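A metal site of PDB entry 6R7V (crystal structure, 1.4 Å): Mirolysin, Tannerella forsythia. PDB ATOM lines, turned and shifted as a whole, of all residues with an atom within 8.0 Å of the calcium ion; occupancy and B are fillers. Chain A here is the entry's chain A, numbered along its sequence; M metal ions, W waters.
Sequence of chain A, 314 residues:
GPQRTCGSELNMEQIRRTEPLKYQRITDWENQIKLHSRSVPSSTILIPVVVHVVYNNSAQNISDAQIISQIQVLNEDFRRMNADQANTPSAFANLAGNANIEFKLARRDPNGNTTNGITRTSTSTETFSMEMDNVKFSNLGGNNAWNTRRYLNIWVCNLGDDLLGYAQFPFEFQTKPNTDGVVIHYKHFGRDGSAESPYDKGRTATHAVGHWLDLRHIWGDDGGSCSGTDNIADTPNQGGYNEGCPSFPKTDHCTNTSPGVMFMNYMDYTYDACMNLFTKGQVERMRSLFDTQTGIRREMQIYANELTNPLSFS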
ATOM      1  N   HIS A 217       6.950   0.108 -24.547  1.00  0.00           N
ATOM      2  CA  HIS A 217       7.619   1.167 -23.798  1.00  0.00           C
ATOM      3  C   HIS A 217       8.007   2.304 -24.720  1.00  0.00           C
ATOM      4  O   HIS A 217       8.541   2.065 -25.811  1.00  0.00           O
ATOM      5  CB  HIS A 217       8.840   0.619 -23.114  1.00  0.00           C
ATOM      6  CG  HIS A 217       8.485  -0.289 -21.993  1.00  0.00           C
ATOM      7  ND1 HIS A 217       9.282  -1.341 -21.655  1.00  0.00           N
ATOM      8  CD2 HIS A 217       7.397  -0.280 -21.194  1.00  0.00           C
ATOM      9  CE1 HIS A 217       8.689  -1.938 -20.633  1.00  0.00           C
ATOM     10  NE2 HIS A 217       7.530  -1.371 -20.344  1.00  0.00           N
ATOM     11  N   ILE A 218       7.745   3.527 -24.270  1.00  0.00           N
ATOM     12  CA  ILE A 218       7.867   4.711 -25.132  1.00  0.00           C
ATOM     13  C   ILE A 218       9.320   4.944 -25.608  1.00  0.00           C
ATOM     14  O   ILE A 218       9.542   5.487 -26.694  1.00  0.00           O
ATOM     15  CB  ILE A 218       7.307   5.935 -24.385  1.00  0.00           C
ATOM     16  CG1 ILE A 218       7.207   7.150 -25.310  1.00  0.00           C
ATOM     17  CG2 ILE A 218       8.123   6.260 -23.104  1.00  0.00           C
ATOM     18  CD1 ILE A 218       6.306   8.253 -24.742  1.00  0.00           C
ATOM     19  N   TRP A 219      10.307   4.515 -24.818  1.00  0.00           N
ATOM     20  CA  TRP A 219      11.708   4.722 -25.196  1.00  0.00           C
ATOM     21  C   TRP A 219      12.269   3.620 -26.117  1.00  0.00           C
ATOM     22  O   TRP A 219      13.447   3.703 -26.524  1.00  0.00           O
ATOM     23  CB  TRP A 219      12.597   4.888 -23.958  1.00  0.00           C
ATOM     24  CG  TRP A 219      12.783   3.630 -23.187  1.00  0.00           C
ATOM     25  CD1 TRP A 219      13.806   2.730 -23.302  1.00  0.00           C
ATOM     26  CD2 TRP A 219      11.880   3.096 -22.209  1.00  0.00           C
ATOM     27  NE1 TRP A 219      13.580   1.665 -22.456  1.00  0.00           N
ATOM     28  CE2 TRP A 219      12.427   1.865 -21.763  1.00  0.00           C
ATOM     29  CE3 TRP A 219      10.703   3.566 -21.608  1.00  0.00           C
ATOM     30  CZ2 TRP A 219      11.797   1.085 -20.782  1.00  0.00           C
ATOM     31  CZ3 TRP A 219      10.084   2.783 -20.647  1.00  0.00           C
ATOM     32  CH2 TRP A 219      10.650   1.562 -20.222  1.00  0.00           C
ATOM     33  N   GLY A 220      11.486   2.596 -26.443  1.00  0.00           N
ATOM     34  CA  GLY A 220      11.931   1.592 -27.400  1.00  0.00           C
ATOM     35  C   GLY A 220      12.738   0.416 -26.907  1.00  0.00           C
ATOM     36  O   GLY A 220      13.227  -0.359 -27.726  1.00  0.00           O
ATOM     37  N   GLY A 228      15.739   2.147 -31.138  1.00  0.00           N
ATOM     38  CA  GLY A 228      14.523   1.416 -30.856  1.00  0.00           C
ATOM     39  C   GLY A 228      13.321   2.299 -31.068  1.00  0.00           C
ATOM     40  O   GLY A 228      13.435   3.525 -31.139  1.00  0.00           O
ATOM     41  N   THR A 229      12.160   1.684 -31.197  1.00  0.00           N
ATOM     42  CA  THR A 229      10.946   2.464 -31.451  1.00  0.00           C
ATOM     43  C   THR A 229       9.786   1.847 -30.742  1.00  0.00           C
ATOM     44  O   THR A 229       9.809   0.648 -30.479  1.00  0.00           O
ATOM     45  CB  THR A 229      10.659   2.517 -32.968  1.00  0.00           C
ATOM     46  OG1 THR A 229       9.489   3.308 -33.217  1.00  0.00           O
ATOM     47  CG2 THR A 229      10.494   1.121 -33.598  1.00  0.00           C
ATOM     48  N   ASP A 230       8.764   2.670 -30.432  1.00  0.00           N
ATOM     49  CA  ASP A 230       7.506   2.142 -29.903  1.00  0.00           C
ATOM     50  C   ASP A 230       6.491   2.049 -31.041  1.00  0.00           C
ATOM     51  O   ASP A 230       5.338   1.707 -30.805  1.00  0.00           O
ATOM     52  CB  ASP A 230       6.992   2.976 -28.712  1.00  0.00           C
ATOM     53  CG  ASP A 230       6.552   4.386 -29.041  1.00  0.00           C
ATOM     54  OD1 ASP A 230       6.928   4.894 -30.128  1.00  0.00           O
ATOM     55  OD2 ASP A 230       5.834   4.987 -28.206  1.00  0.00           O
ATOM     56  N   ASN A 231       6.918   2.325 -32.293  1.00  0.00           N
ATOM     57  CA  ASN A 231       6.063   2.272 -33.495  1.00  0.00           C
ATOM     58  C   ASN A 231       4.921   3.294 -33.451  1.00  0.00           C
ATOM     59  O   ASN A 231       3.956   3.146 -34.197  1.00  0.00           O
ATOM     60  CB  ASN A 231       5.513   0.869 -33.784  1.00  0.00           C
ATOM     61  CG  ASN A 231       6.609  -0.161 -33.930  1.00  0.00           C
ATOM     62  OD1 ASN A 231       6.631  -1.155 -33.210  1.00  0.00           O
ATOM     63  ND2 ASN A 231       7.570   0.080 -34.809  1.00  0.00           N
ATOM     64  N   ILE A 232       5.053   4.338 -32.617  1.00  0.00           N
ATOM     65  CA  ILE A 232       4.060   5.414 -32.542  1.00  0.00           C
ATOM     66  C   ILE A 232       4.718   6.730 -32.972  1.00  0.00           C
ATOM     67  O   ILE A 232       5.646   7.203 -32.306  1.00  0.00           O
ATOM     68  CB  ILE A 232       3.432   5.524 -31.139  1.00  0.00           C
ATOM     69  CG1 ILE A 232       2.887   4.159 -30.598  1.00  0.00           C
ATOM     70  CG2 ILE A 232       2.346   6.602 -31.148  1.00  0.00           C
ATOM     71  CD1 ILE A 232       1.680   3.601 -31.313  1.00  0.00           C
ATOM     72  N   ALA A 233       4.233   7.321 -34.086  1.00  0.00           N
ATOM     73  CA  ALA A 233       4.862   8.535 -34.572  1.00  0.00           C
ATOM     74  C   ALA A 233       4.683   9.760 -33.661  1.00  0.00           C
ATOM     75  O   ALA A 233       5.585  10.608 -33.613  1.00  0.00           O
ATOM     76  CB  ALA A 233       4.325   8.863 -35.974  1.00  0.00           C
ATOM     77  N   ASP A 234       3.555   9.838 -32.899  1.00  0.00           N
ATOM     78  CA  ASP A 234       3.356  11.059 -32.108  1.00  0.00           C
ATOM     79  C   ASP A 234       3.940  10.958 -30.680  1.00  0.00           C
ATOM     80  O   ASP A 234       3.849  11.935 -29.923  1.00  0.00           O
ATOM     81  CB  ASP A 234       1.899  11.503 -32.086  1.00  0.00           C
ATOM     82  CG  ASP A 234       0.949  10.554 -31.426  1.00  0.00           C
ATOM     83  OD1 ASP A 234       1.416   9.546 -30.846  1.00  0.00           O
ATOM     84  OD2 ASP A 234      -0.272  10.838 -31.428  1.00  0.00           O
ATOM     85  N   THR A 235       4.641   9.835 -30.346  1.00  0.00           N
ATOM     86  CA  THR A 235       5.412   9.797 -29.105  1.00  0.00           C
ATOM     87  C   THR A 235       6.856  10.178 -29.525  1.00  0.00           C
ATOM     88  O   THR A 235       7.452   9.479 -30.371  1.00  0.00           O
ATOM     89  CB  THR A 235       5.325   8.450 -28.379  1.00  0.00           C
ATOM     90  OG1 THR A 235       5.646   7.440 -29.338  1.00  0.00           O
ATOM     91  CG2 THR A 235       3.967   8.221 -27.772  1.00  0.00           C
ATOM     92  N   PRO A 236       7.397  11.283 -28.973  1.00  0.00           N
ATOM     93  CA  PRO A 236       8.766  11.691 -29.353  1.00  0.00           C
ATOM     94  C   PRO A 236       9.783  10.569 -29.155  1.00  0.00           C
ATOM     95  O   PRO A 236       9.700   9.858 -28.157  1.00  0.00           O
ATOM     96  CB  PRO A 236       9.075  12.837 -28.399  1.00  0.00           C
ATOM     97  CG  PRO A 236       7.721  13.402 -28.018  1.00  0.00           C
ATOM     98  CD  PRO A 236       6.805  12.208 -27.971  1.00  0.00           C
ATOM     99  N   ASN A 237      10.746  10.436 -30.092  1.00  0.00           N
ATOM    100  CA  ASN A 237      11.837   9.479 -29.971  1.00  0.00           C
ATOM    101  C   ASN A 237      12.542   9.749 -28.658  1.00  0.00           C
ATOM    102  O   ASN A 237      12.811  10.900 -28.307  1.00  0.00           O
ATOM    103  CB  ASN A 237      12.807   9.596 -31.135  1.00  0.00           C
ATOM    104  CG  ASN A 237      13.793   8.474 -31.265  1.00  0.00           C
ATOM    105  OD1 ASN A 237      13.888   7.575 -30.438  1.00  0.00           O
ATOM    106  ND2 ASN A 237      14.564   8.496 -32.340  1.00  0.00           N
ATOM    107  N   GLN A 238      12.783   8.714 -27.898  1.00  0.00           N
ATOM    108  CA  GLN A 238      13.281   8.887 -26.546  1.00  0.00           C
ATOM    109  C   GLN A 238      14.443   7.932 -26.302  1.00  0.00           C
ATOM    110  O   GLN A 238      14.402   6.812 -26.786  1.00  0.00           O
ATOM    111  CB  GLN A 238      12.091   8.608 -25.580  1.00  0.00           C
ATOM    112  CG  GLN A 238      12.400   8.695 -24.083  1.00  0.00           C
ATOM    113  CD  GLN A 238      11.163   8.593 -23.226  1.00  0.00           C
ATOM    114  OE1 GLN A 238      10.091   9.089 -23.540  1.00  0.00           O
ATOM    115  NE2 GLN A 238      11.286   7.925 -22.106  1.00  0.00           N
ATOM    116  N   THR A 279      -1.319   8.944 -26.133  1.00  0.00           N
ATOM    117  CA  THR A 279      -1.453   9.817 -27.305  1.00  0.00           C
ATOM    118  C   THR A 279      -2.559   9.318 -28.244  1.00  0.00           C
ATOM    119  O   THR A 279      -2.983   8.145 -28.164  1.00  0.00           O
ATOM    120  CB  THR A 279      -0.158   9.903 -28.101  1.00  0.00           C
ATOM    121  OG1 THR A 279       0.113   8.653 -28.739  1.00  0.00           O
ATOM    122  CG2 THR A 279       1.014  10.375 -27.313  1.00  0.00           C
ATOM    123  N   GLN A 282      -1.242   6.177 -29.936  1.00  0.00           N
ATOM    124  CA  GLN A 282      -1.341   4.981 -29.101  1.00  0.00           C
ATOM    125  C   GLN A 282      -2.788   4.485 -29.086  1.00  0.00           C
ATOM    126  O   GLN A 282      -2.990   3.291 -29.224  1.00  0.00           O
ATOM    127  CB  GLN A 282      -0.852   5.277 -27.676  1.00  0.00           C
ATOM    128  CG  GLN A 282       0.672   5.449 -27.588  1.00  0.00           C
ATOM    129  CD  GLN A 282       1.063   5.944 -26.211  1.00  0.00           C
ATOM    130  OE1 GLN A 282       0.395   6.814 -25.628  1.00  0.00           O
ATOM    131  NE2 GLN A 282       2.131   5.358 -25.641  1.00  0.00           N
HETATM  132 CA    CA M   1       7.589   7.077 -30.897  1.00  0.00          CA
HETATM  133  O   HOH W   1       9.809   5.807 -30.827  1.00  0.00           O
HETATM  134  O   HOH W   2       8.635   7.347 -28.663  1.00  0.00           O
HETATM  135  O   HOH W   3       7.931   5.596 -32.945  1.00  0.00           O
HETATM  136  O   HOH W   4       8.949   8.249 -32.436  1.00  0.00           O
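Water W2 lies within hydrogen-bond range of the backbone carbonyl oxygen (O) of Pro 236 and the backbone carbonyl oxygen (O) of Ile 218. Water W3 lies within hydrogen-bond range of OG1 of Thr 229, N of Ile 232 and N of Asn 231. Water W1 bridges the backbone NH of Asp 230 (3.3 Å) and the side-chain hydroxyl of Thr 229 (3.5 Å).
The calcium ion is bound by water W4 (2.4 Å), the backbone carbonyl oxygen of Ile 232 (2.4 Å), the side-chain carboxylate of Asp 230 (2.4 Å), the backbone carbonyl oxygen of Thr 235 (2.5 Å), water W2 (2.5 Å), the side-chain hydroxyl of Thr 235 (2.5 Å), water W3 (2.6 Å) and water W1 (2.6 Å). The calcium ion has eight donor atoms within binding distance.
Within 4 Å of the calcium ion: Asp 230, Ile 232 and Thr 235. The nearest printed residue that does not touch the calcium ion is Pro 236 (4.4 Å).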
